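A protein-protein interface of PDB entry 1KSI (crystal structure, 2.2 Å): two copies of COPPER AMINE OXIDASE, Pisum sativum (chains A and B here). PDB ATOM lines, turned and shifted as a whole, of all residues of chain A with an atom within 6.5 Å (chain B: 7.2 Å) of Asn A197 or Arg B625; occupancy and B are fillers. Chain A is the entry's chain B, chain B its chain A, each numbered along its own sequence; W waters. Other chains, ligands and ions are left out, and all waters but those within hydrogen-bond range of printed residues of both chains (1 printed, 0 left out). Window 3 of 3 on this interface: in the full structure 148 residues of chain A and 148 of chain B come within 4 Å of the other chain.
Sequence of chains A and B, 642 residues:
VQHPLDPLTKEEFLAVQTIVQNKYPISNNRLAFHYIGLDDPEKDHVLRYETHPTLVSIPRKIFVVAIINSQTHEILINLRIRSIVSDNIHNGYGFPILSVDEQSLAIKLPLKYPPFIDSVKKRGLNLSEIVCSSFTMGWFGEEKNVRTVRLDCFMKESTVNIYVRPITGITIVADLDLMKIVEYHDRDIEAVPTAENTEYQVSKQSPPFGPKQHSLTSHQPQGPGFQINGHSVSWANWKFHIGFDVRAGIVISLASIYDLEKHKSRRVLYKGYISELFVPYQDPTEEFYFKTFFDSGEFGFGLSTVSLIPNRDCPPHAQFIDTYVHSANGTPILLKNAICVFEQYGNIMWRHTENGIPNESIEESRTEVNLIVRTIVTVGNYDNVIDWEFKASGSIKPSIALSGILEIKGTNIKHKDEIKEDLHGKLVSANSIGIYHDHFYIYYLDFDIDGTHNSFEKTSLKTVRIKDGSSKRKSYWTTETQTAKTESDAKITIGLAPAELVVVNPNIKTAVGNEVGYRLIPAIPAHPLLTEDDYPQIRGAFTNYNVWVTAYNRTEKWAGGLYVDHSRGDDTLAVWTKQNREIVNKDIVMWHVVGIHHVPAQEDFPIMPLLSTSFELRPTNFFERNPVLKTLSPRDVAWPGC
Of the 14 printed residues of chain A, 6 touch a printed residue of chain B.
Hydrophobic or aromatic side chains of chain A that line the printed part of chain B: Pro A606.
Along chain A the printed residues that touch a printed residue of chain B span positions 197 to 606.
Printed residues of chain B that touch a printed residue of chain A: Thr B510, Phe B622, Phe B623, Glu B624, Arg B625, Asn B626 and Leu B629.
Among the printed residues, no Asp or Glu carboxylate lies within 4 Å of a Lys or Arg side-chain nitrogen of the other chain.
Among the printed residues, pairs that only touch across the chains: Gln A602 with Arg B625 (2.9 Å), Glu A603 with Asn B626 (3.2 Å), Phe A605 with Arg B625 (3.3 Å), Gln A602 with Phe B623 (3.6 Å), Glu A199 with Leu B629 (3.7 Å), Glu A603 with Arg B625 (3.8 Å), Asn A197 with Arg B625 (3.9 Å) and Pro A606 with Leu B629 (3.9 Å).
No position is printed for both chains.
Asn A197 touches just one residue of chain B: Arg B625 (3.9 Å).
Arg B625 touches just these residues of chain A: Asn A197, Gln A602, Glu A603 and Phe A605.
Of the printed residues of chain B, Glu A199 touches Leu B629.
Of the printed residues of chain A, Phe B623 touches Gln A602 and Glu A603.
Asp A604 touches none of the printed residues of chain B.
Asp B259 touches none of the printed residues of chain A.
The nearest printed residue of chain A that does not touch Thr B510 is Glu A603 (6.9 Å).
The side-chain amide oxygen (OD1) of Asn B626 is in hydrogen-bond range of the backbone NH (N) of Leu B629, 3.3 Å away.
The side-chain amide oxygen of Asn B626 lies within hydrogen-bond range of the backbone NH of Val B628, 2.8 Å away.
The guanidinium group of Arg B625 is in salt-bridge range of the side-chain carboxylate of Glu B261 (3.0 Å).
OE1 of Glu B624 is in hydrogen-bond range of N of Ala B511, at 3.1 Å.
The backbone carbonyl oxygen (O) of Pro A606 lies within hydrogen-bond range of the side-chain amide nitrogen (ND2) of Asn A161, 3.4 Å away.
The backbone NH (N) of Phe B623 lies within hydrogen-bond range of the side-chain carboxylate (OE2) of Glu A603.
The backbone NH (N) of Phe B622 is in hydrogen-bond range of the side-chain carboxylate (OE2) of Glu A603 (2.6 Å).
The side-chain amide oxygen (OE1) of Gln A602 sits at hydrogen-bond distance from the side-chain hydroxyl (OG1) of Thr B510 (2.7 Å).
The backbone carbonyl oxygen (O) of Glu B624 lies within hydrogen-bond range of the side-chain amide nitrogen (NE2) of Gln A602 (2.8 Å).
O of Phe A605 is in hydrogen-bond range of N of Asn B626 (2.9 Å).
The backbone NH (N) of Asn B626 sits at hydrogen-bond distance from the backbone carbonyl oxygen (O) of Gln A602 (3.4 Å).
Water W1 lies within hydrogen-bond range of O of Val A428 (2.7 Å), O of Glu B624 (2.9 Å) and OG of Ser A429 (3.4 Å).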
ATOM      1  N   ASN A 161       5.976  -7.501   9.220  1.00  0.00           N
ATOM      2  CA  ASN A 161       4.960  -7.033   8.279  1.00  0.00           C
ATOM      3  C   ASN A 161       5.212  -5.595   7.861  1.00  0.00           C
ATOM      4  O   ASN A 161       4.507  -4.639   8.214  1.00  0.00           O
ATOM      5  CB  ASN A 161       3.594  -7.263   8.952  1.00  0.00           C
ATOM      6  CG  ASN A 161       2.462  -7.361   7.936  1.00  0.00           C
ATOM      7  OD1 ASN A 161       2.613  -6.950   6.780  1.00  0.00           O
ATOM      8  ND2 ASN A 161       1.313  -7.895   8.373  1.00  0.00           N
ATOM      9  N   THR A 194       1.220   1.675  13.603  1.00  0.00           N
ATOM     10  CA  THR A 194       1.824   0.855  14.643  1.00  0.00           C
ATOM     11  C   THR A 194       2.144  -0.569  14.224  1.00  0.00           C
ATOM     12  O   THR A 194       1.595  -1.154  13.288  1.00  0.00           O
ATOM     13  CB  THR A 194       0.894   0.707  15.866  1.00  0.00           C
ATOM     14  OG1 THR A 194       1.546  -0.061  16.893  1.00  0.00           O
ATOM     15  CG2 THR A 194      -0.414   0.007  15.492  1.00  0.00           C
ATOM     16  N   ALA A 195       3.085  -1.166  14.944  1.00  0.00           N
ATOM     17  CA  ALA A 195       3.472  -2.537  14.652  1.00  0.00           C
ATOM     18  C   ALA A 195       2.557  -3.545  15.368  1.00  0.00           C
ATOM     19  O   ALA A 195       2.602  -4.749  15.117  1.00  0.00           O
ATOM     20  CB  ALA A 195       4.898  -2.780  15.100  1.00  0.00           C
ATOM     21  N   GLU A 196       1.737  -3.116  16.272  1.00  0.00           N
ATOM     22  CA  GLU A 196       0.899  -3.962  17.141  1.00  0.00           C
ATOM     23  C   GLU A 196      -0.164  -4.718  16.370  1.00  0.00           C
ATOM     24  O   GLU A 196      -0.908  -4.050  15.652  1.00  0.00           O
ATOM     25  CB  GLU A 196       0.256  -2.896  18.017  1.00  0.00           C
ATOM     26  CG  GLU A 196      -0.708  -3.288  19.072  1.00  0.00           C
ATOM     27  CD  GLU A 196       0.013  -3.235  20.431  1.00  0.00           C
ATOM     28  OE1 GLU A 196       1.069  -3.921  20.478  1.00  0.00           O
ATOM     29  OE2 GLU A 196      -0.528  -2.508  21.314  1.00  0.00           O
ATOM     30  N   ASN A 197      -0.239  -6.034  16.453  1.00  0.00           N
ATOM     31  CA  ASN A 197      -1.244  -6.820  15.731  1.00  0.00           C
ATOM     32  C   ASN A 197      -1.079  -6.941  14.229  1.00  0.00           C
ATOM     33  O   ASN A 197      -2.117  -6.976  13.530  1.00  0.00           O
ATOM     34  CB  ASN A 197      -2.673  -6.262  15.922  1.00  0.00           C
ATOM     35  CG  ASN A 197      -3.055  -6.283  17.388  1.00  0.00           C
ATOM     36  OD1 ASN A 197      -3.549  -5.252  17.848  1.00  0.00           O
ATOM     37  ND2 ASN A 197      -2.783  -7.384  18.082  1.00  0.00           N
ATOM     38  N   THR A 198       0.167  -6.991  13.747  1.00  0.00           N
ATOM     39  CA  THR A 198       0.412  -6.976  12.300  1.00  0.00           C
ATOM     40  C   THR A 198       1.175  -8.244  11.945  1.00  0.00           C
ATOM     41  O   THR A 198       1.269  -8.636  10.791  1.00  0.00           O
ATOM     42  CB  THR A 198       1.278  -5.760  11.874  1.00  0.00           C
ATOM     43  OG1 THR A 198       2.537  -5.824  12.590  1.00  0.00           O
ATOM     44  CG2 THR A 198       0.618  -4.416  12.107  1.00  0.00           C
ATOM     45  N   GLU A 199       1.721  -8.870  12.953  1.00  0.00           N
ATOM     46  CA  GLU A 199       2.478 -10.115  12.815  1.00  0.00           C
ATOM     47  C   GLU A 199       1.582 -11.323  12.470  1.00  0.00           C
ATOM     48  O   GLU A 199       0.433 -11.452  12.937  1.00  0.00           O
ATOM     49  CB  GLU A 199       3.229 -10.343  14.115  1.00  0.00           C
ATOM     50  CG  GLU A 199       4.311 -11.374  14.140  1.00  0.00           C
ATOM     51  CD  GLU A 199       5.410 -11.228  13.082  1.00  0.00           C
ATOM     52  OE1 GLU A 199       6.263 -10.320  13.319  1.00  0.00           O
ATOM     53  OE2 GLU A 199       5.314 -12.063  12.121  1.00  0.00           O
ATOM     54  N   VAL A 428      -8.624   0.831   6.954  1.00  0.00           N
ATOM     55  CA  VAL A 428      -8.801  -0.532   7.438  1.00  0.00           C
ATOM     56  C   VAL A 428      -8.166  -0.720   8.792  1.00  0.00           C
ATOM     57  O   VAL A 428      -8.215  -1.797   9.419  1.00  0.00           O
ATOM     58  CB  VAL A 428      -8.173  -1.541   6.445  1.00  0.00           C
ATOM     59  CG1 VAL A 428      -8.869  -1.422   5.090  1.00  0.00           C
ATOM     60  CG2 VAL A 428      -6.674  -1.250   6.327  1.00  0.00           C
ATOM     61  N   SER A 429      -7.542   0.369   9.245  1.00  0.00           N
ATOM     62  CA  SER A 429      -6.901   0.343  10.582  1.00  0.00           C
ATOM     63  C   SER A 429      -6.512   1.784  10.886  1.00  0.00           C
ATOM     64  O   SER A 429      -6.536   2.598   9.922  1.00  0.00           O
ATOM     65  CB  SER A 429      -5.729  -0.585  10.646  1.00  0.00           C
ATOM     66  OG  SER A 429      -5.313  -0.862  11.987  1.00  0.00           O
ATOM     67  N   GLN A 602     -11.645  -4.469   6.560  1.00  0.00           N
ATOM     68  CA  GLN A 602     -10.688  -4.736   7.656  1.00  0.00           C
ATOM     69  C   GLN A 602     -10.312  -6.155   7.843  1.00  0.00           C
ATOM     70  O   GLN A 602      -9.406  -6.456   8.618  1.00  0.00           O
ATOM     71  CB  GLN A 602     -11.307  -4.210   8.976  1.00  0.00           C
ATOM     72  CG  GLN A 602     -11.766  -2.751   8.802  1.00  0.00           C
ATOM     73  CD  GLN A 602     -12.201  -2.130  10.111  1.00  0.00           C
ATOM     74  OE1 GLN A 602     -13.034  -1.193  10.089  1.00  0.00           O
ATOM     75  NE2 GLN A 602     -11.682  -2.591  11.239  1.00  0.00           N
ATOM     76  N   GLU A 603     -11.037  -7.118   7.257  1.00  0.00           N
ATOM     77  CA  GLU A 603     -10.725  -8.544   7.366  1.00  0.00           C
ATOM     78  C   GLU A 603      -9.529  -8.863   6.459  1.00  0.00           C
ATOM     79  O   GLU A 603      -8.865  -9.888   6.643  1.00  0.00           O
ATOM     80  CB  GLU A 603     -11.951  -9.415   6.956  1.00  0.00           C
ATOM     81  CG  GLU A 603     -13.203  -9.332   7.830  1.00  0.00           C
ATOM     82  CD  GLU A 603     -14.165  -8.203   7.620  1.00  0.00           C
ATOM     83  OE1 GLU A 603     -14.043  -7.234   6.806  1.00  0.00           O
ATOM     84  OE2 GLU A 603     -15.214  -8.194   8.369  1.00  0.00           O
ATOM     85  N   ASP A 604      -9.271  -8.044   5.434  1.00  0.00           N
ATOM     86  CA  ASP A 604      -8.094  -8.166   4.576  1.00  0.00           C
ATOM     87  C   ASP A 604      -6.782  -7.850   5.316  1.00  0.00           C
ATOM     88  O   ASP A 604      -5.711  -8.215   4.824  1.00  0.00           O
ATOM     89  CB  ASP A 604      -8.166  -7.217   3.384  1.00  0.00           C
ATOM     90  CG  ASP A 604      -9.261  -7.476   2.385  1.00  0.00           C
ATOM     91  OD1 ASP A 604      -9.766  -8.637   2.370  1.00  0.00           O
ATOM     92  OD2 ASP A 604      -9.641  -6.608   1.545  1.00  0.00           O
ATOM     93  N   PHE A 605      -6.794  -7.214   6.469  1.00  0.00           N
ATOM     94  CA  PHE A 605      -5.672  -6.743   7.268  1.00  0.00           C
ATOM     95  C   PHE A 605      -5.439  -7.516   8.527  1.00  0.00           C
ATOM     96  O   PHE A 605      -6.441  -7.860   9.178  1.00  0.00           O
ATOM     97  CB  PHE A 605      -6.132  -5.297   7.689  1.00  0.00           C
ATOM     98  CG  PHE A 605      -5.070  -4.591   8.493  1.00  0.00           C
ATOM     99  CD1 PHE A 605      -4.066  -3.856   7.846  1.00  0.00           C
ATOM    100  CD2 PHE A 605      -5.027  -4.707   9.867  1.00  0.00           C
ATOM    101  CE1 PHE A 605      -3.079  -3.211   8.560  1.00  0.00           C
ATOM    102  CE2 PHE A 605      -4.037  -4.097  10.604  1.00  0.00           C
ATOM    103  CZ  PHE A 605      -3.049  -3.336   9.948  1.00  0.00           C
ATOM    104  N   PRO A 606      -4.226  -7.774   8.988  1.00  0.00           N
ATOM    105  CA  PRO A 606      -2.992  -7.353   8.389  1.00  0.00           C
ATOM    106  C   PRO A 606      -2.503  -8.287   7.283  1.00  0.00           C
ATOM    107  O   PRO A 606      -1.528  -8.030   6.571  1.00  0.00           O
ATOM    108  CB  PRO A 606      -1.982  -7.473   9.567  1.00  0.00           C
ATOM    109  CG  PRO A 606      -2.471  -8.582  10.420  1.00  0.00           C
ATOM    110  CD  PRO A 606      -3.973  -8.505  10.283  1.00  0.00           C
ATOM    111  N   ASP B 259     -16.842 -14.099  18.105  1.00  0.00           N
ATOM    112  CA  ASP B 259     -15.764 -13.149  17.801  1.00  0.00           C
ATOM    113  C   ASP B 259     -14.732 -13.257  18.912  1.00  0.00           C
ATOM    114  O   ASP B 259     -14.928 -12.788  20.037  1.00  0.00           O
ATOM    115  CB  ASP B 259     -16.319 -11.736  17.760  1.00  0.00           C
ATOM    116  CG  ASP B 259     -15.397 -10.712  17.103  1.00  0.00           C
ATOM    117  OD1 ASP B 259     -14.163 -10.821  17.357  1.00  0.00           O
ATOM    118  OD2 ASP B 259     -15.896  -9.806  16.393  1.00  0.00           O
ATOM    119  N   GLU B 261     -12.016 -11.773  19.430  1.00  0.00           N
ATOM    120  CA  GLU B 261     -11.420 -10.505  19.778  1.00  0.00           C
ATOM    121  C   GLU B 261     -12.387  -9.731  20.642  1.00  0.00           C
ATOM    122  O   GLU B 261     -11.964  -9.136  21.616  1.00  0.00           O
ATOM    123  CB  GLU B 261     -11.162  -9.689  18.505  1.00  0.00           C
ATOM    124  CG  GLU B 261      -9.970  -8.753  18.419  1.00  0.00           C
ATOM    125  CD  GLU B 261     -10.301  -7.272  18.427  1.00  0.00           C
ATOM    126  OE1 GLU B 261     -11.516  -6.928  18.587  1.00  0.00           O
ATOM    127  OE2 GLU B 261      -9.400  -6.390  18.273  1.00  0.00           O
ATOM    128  N   THR B 510     -16.925  -0.478  13.682  1.00  0.00           N
ATOM    129  CA  THR B 510     -15.621  -0.915  14.198  1.00  0.00           C
ATOM    130  C   THR B 510     -14.890   0.247  14.910  1.00  0.00           C
ATOM    131  O   THR B 510     -15.260   1.422  14.877  1.00  0.00           O
ATOM    132  CB  THR B 510     -14.768  -1.402  13.009  1.00  0.00           C
ATOM    133  OG1 THR B 510     -14.644  -0.298  12.087  1.00  0.00           O
ATOM    134  CG2 THR B 510     -15.472  -2.536  12.252  1.00  0.00           C
ATOM    135  N   ALA B 511     -13.786  -0.087  15.596  1.00  0.00           N
ATOM    136  CA  ALA B 511     -12.984   0.966  16.244  1.00  0.00           C
ATOM    137  C   ALA B 511     -12.673   2.103  15.261  1.00  0.00           C
ATOM    138  O   ALA B 511     -12.766   3.300  15.613  1.00  0.00           O
ATOM    139  CB  ALA B 511     -11.832   0.315  16.955  1.00  0.00           C
ATOM    140  N   PHE B 622     -16.943  -6.525   9.355  1.00  0.00           N
ATOM    141  CA  PHE B 622     -17.744  -7.109  10.445  1.00  0.00           C
ATOM    142  C   PHE B 622     -16.832  -7.294  11.629  1.00  0.00           C
ATOM    143  O   PHE B 622     -17.131  -7.091  12.785  1.00  0.00           O
ATOM    144  CB  PHE B 622     -18.373  -8.450   9.942  1.00  0.00           C
ATOM    145  CG  PHE B 622     -19.340  -9.115  10.925  1.00  0.00           C
ATOM    146  CD1 PHE B 622     -20.692  -8.727  10.973  1.00  0.00           C
ATOM    147  CD2 PHE B 622     -18.926 -10.138  11.760  1.00  0.00           C
ATOM    148  CE1 PHE B 622     -21.566  -9.311  11.862  1.00  0.00           C
ATOM    149  CE2 PHE B 622     -19.776 -10.748  12.671  1.00  0.00           C
ATOM    150  CZ  PHE B 622     -21.094 -10.316  12.713  1.00  0.00           C
ATOM    151  N   PHE B 623     -15.620  -7.775  11.372  1.00  0.00           N
ATOM    152  CA  PHE B 623     -14.528  -7.997  12.304  1.00  0.00           C
ATOM    153  C   PHE B 623     -13.486  -6.850  12.268  1.00  0.00           C
ATOM    154  O   PHE B 623     -13.331  -6.168  11.263  1.00  0.00           O
ATOM    155  CB  PHE B 623     -13.760  -9.310  12.042  1.00  0.00           C
ATOM    156  CG  PHE B 623     -14.680 -10.512  12.061  1.00  0.00           C
ATOM    157  CD1 PHE B 623     -15.129 -11.068  13.246  1.00  0.00           C
ATOM    158  CD2 PHE B 623     -15.099 -11.065  10.849  1.00  0.00           C
ATOM    159  CE1 PHE B 623     -15.964 -12.181  13.193  1.00  0.00           C
ATOM    160  CE2 PHE B 623     -15.929 -12.164  10.766  1.00  0.00           C
ATOM    161  CZ  PHE B 623     -16.361 -12.715  11.962  1.00  0.00           C
ATOM    162  N   GLU B 624     -12.816  -6.682  13.405  1.00  0.00           N
ATOM    163  CA  GLU B 624     -11.859  -5.611  13.566  1.00  0.00           C
ATOM    164  C   GLU B 624     -10.688  -5.799  12.597  1.00  0.00           C
ATOM    165  O   GLU B 624     -10.213  -4.790  12.033  1.00  0.00           O
ATOM    166  CB  GLU B 624     -11.381  -5.439  14.997  1.00  0.00           C
ATOM    167  CG  GLU B 624     -10.850  -4.020  15.212  1.00  0.00           C
ATOM    168  CD  GLU B 624     -11.859  -2.867  15.058  1.00  0.00           C
ATOM    169  OE1 GLU B 624     -12.901  -3.003  15.779  1.00  0.00           O
ATOM    170  OE2 GLU B 624     -11.552  -1.907  14.262  1.00  0.00           O
ATOM    171  N   ARG B 625     -10.346  -7.038  12.326  1.00  0.00           N
ATOM    172  CA  ARG B 625      -9.299  -7.400  11.396  1.00  0.00           C
ATOM    173  C   ARG B 625      -9.478  -8.860  10.991  1.00  0.00           C
ATOM    174  O   ARG B 625     -10.370  -9.472  11.570  1.00  0.00           O
ATOM    175  CB  ARG B 625      -7.924  -7.280  12.096  1.00  0.00           C
ATOM    176  CG  ARG B 625      -7.664  -8.142  13.299  1.00  0.00           C
ATOM    177  CD  ARG B 625      -6.447  -7.611  14.079  1.00  0.00           C
ATOM    178  NE  ARG B 625      -6.699  -6.210  14.478  1.00  0.00           N
ATOM    179  CZ  ARG B 625      -6.935  -5.861  15.744  1.00  0.00           C
ATOM    180  NH1 ARG B 625      -6.905  -6.805  16.700  1.00  0.00           N
ATOM    181  NH2 ARG B 625      -7.205  -4.599  16.052  1.00  0.00           N
ATOM    182  N   ASN B 626      -8.673  -9.423  10.126  1.00  0.00           N
ATOM    183  CA  ASN B 626      -8.729 -10.821   9.755  1.00  0.00           C
ATOM    184  C   ASN B 626      -9.105 -11.715  10.945  1.00  0.00           C
ATOM    185  O   ASN B 626      -8.332 -11.927  11.886  1.00  0.00           O
ATOM    186  CB  ASN B 626      -7.389 -11.218   9.136  1.00  0.00           C
ATOM    187  CG  ASN B 626      -7.257 -12.664   8.778  1.00  0.00           C
ATOM    188  OD1 ASN B 626      -8.014 -13.551   9.188  1.00  0.00           O
ATOM    189  ND2 ASN B 626      -6.256 -13.070   8.004  1.00  0.00           N
ATOM    190  N   PRO B 627     -10.297 -12.354  10.884  1.00  0.00           N
ATOM    191  CA  PRO B 627     -10.823 -13.167  11.983  1.00  0.00           C
ATOM    192  C   PRO B 627     -10.097 -14.469  12.191  1.00  0.00           C
ATOM    193  O   PRO B 627     -10.185 -15.056  13.269  1.00  0.00           O
ATOM    194  CB  PRO B 627     -12.293 -13.362  11.626  1.00  0.00           C
ATOM    195  CG  PRO B 627     -12.259 -13.357  10.108  1.00  0.00           C
ATOM    196  CD  PRO B 627     -11.231 -12.276   9.740  1.00  0.00           C
ATOM    197  N   VAL B 628      -9.364 -14.950  11.182  1.00  0.00           N
ATOM    198  CA  VAL B 628      -8.581 -16.168  11.362  1.00  0.00           C
ATOM    199  C   VAL B 628      -7.089 -15.842  11.500  1.00  0.00           C
ATOM    200  O   VAL B 628      -6.247 -16.690  11.207  1.00  0.00           O
ATOM    201  CB  VAL B 628      -8.859 -17.161  10.198  1.00  0.00           C
ATOM    202  CG1 VAL B 628     -10.238 -17.835  10.493  1.00  0.00           C
ATOM    203  CG2 VAL B 628      -8.993 -16.545   8.838  1.00  0.00           C
ATOM    204  N   LEU B 629      -6.739 -14.628  11.977  1.00  0.00           N
ATOM    205  CA  LEU B 629      -5.329 -14.280  12.166  1.00  0.00           C
ATOM    206  C   LEU B 629      -4.748 -15.221  13.190  1.00  0.00           C
ATOM    207  O   LEU B 629      -3.611 -15.741  13.038  1.00  0.00           O
ATOM    208  CB  LEU B 629      -5.182 -12.813  12.549  1.00  0.00           C
ATOM    209  CG  LEU B 629      -3.693 -12.343  12.808  1.00  0.00           C
ATOM    210  CD1 LEU B 629      -2.902 -12.344  11.524  1.00  0.00           C
ATOM    211  CD2 LEU B 629      -3.741 -10.989  13.480  1.00  0.00           C
ATOM    212  N   LYS B 630      -5.509 -15.587  14.235  1.00  0.00           N
ATOM    213  CA  LYS B 630      -5.049 -16.527  15.252  1.00  0.00           C
ATOM    214  C   LYS B 630      -5.520 -17.962  15.089  1.00  0.00           C
ATOM    215  O   LYS B 630      -5.397 -18.723  16.043  1.00  0.00           O
ATOM    216  CB  LYS B 630      -5.422 -16.091  16.691  1.00  0.00           C
ATOM    217  CG  LYS B 630      -5.279 -14.585  16.826  1.00  0.00           C
ATOM    218  CD  LYS B 630      -3.793 -14.186  16.726  1.00  0.00           C
ATOM    219  CE  LYS B 630      -2.940 -14.885  17.762  1.00  0.00           C
ATOM    220  NZ  LYS B 630      -3.168 -14.362  19.136  1.00  0.00           N
HETATM  221  O   HOH W   1      -7.806  -3.141  11.745  1.00  0.00           O
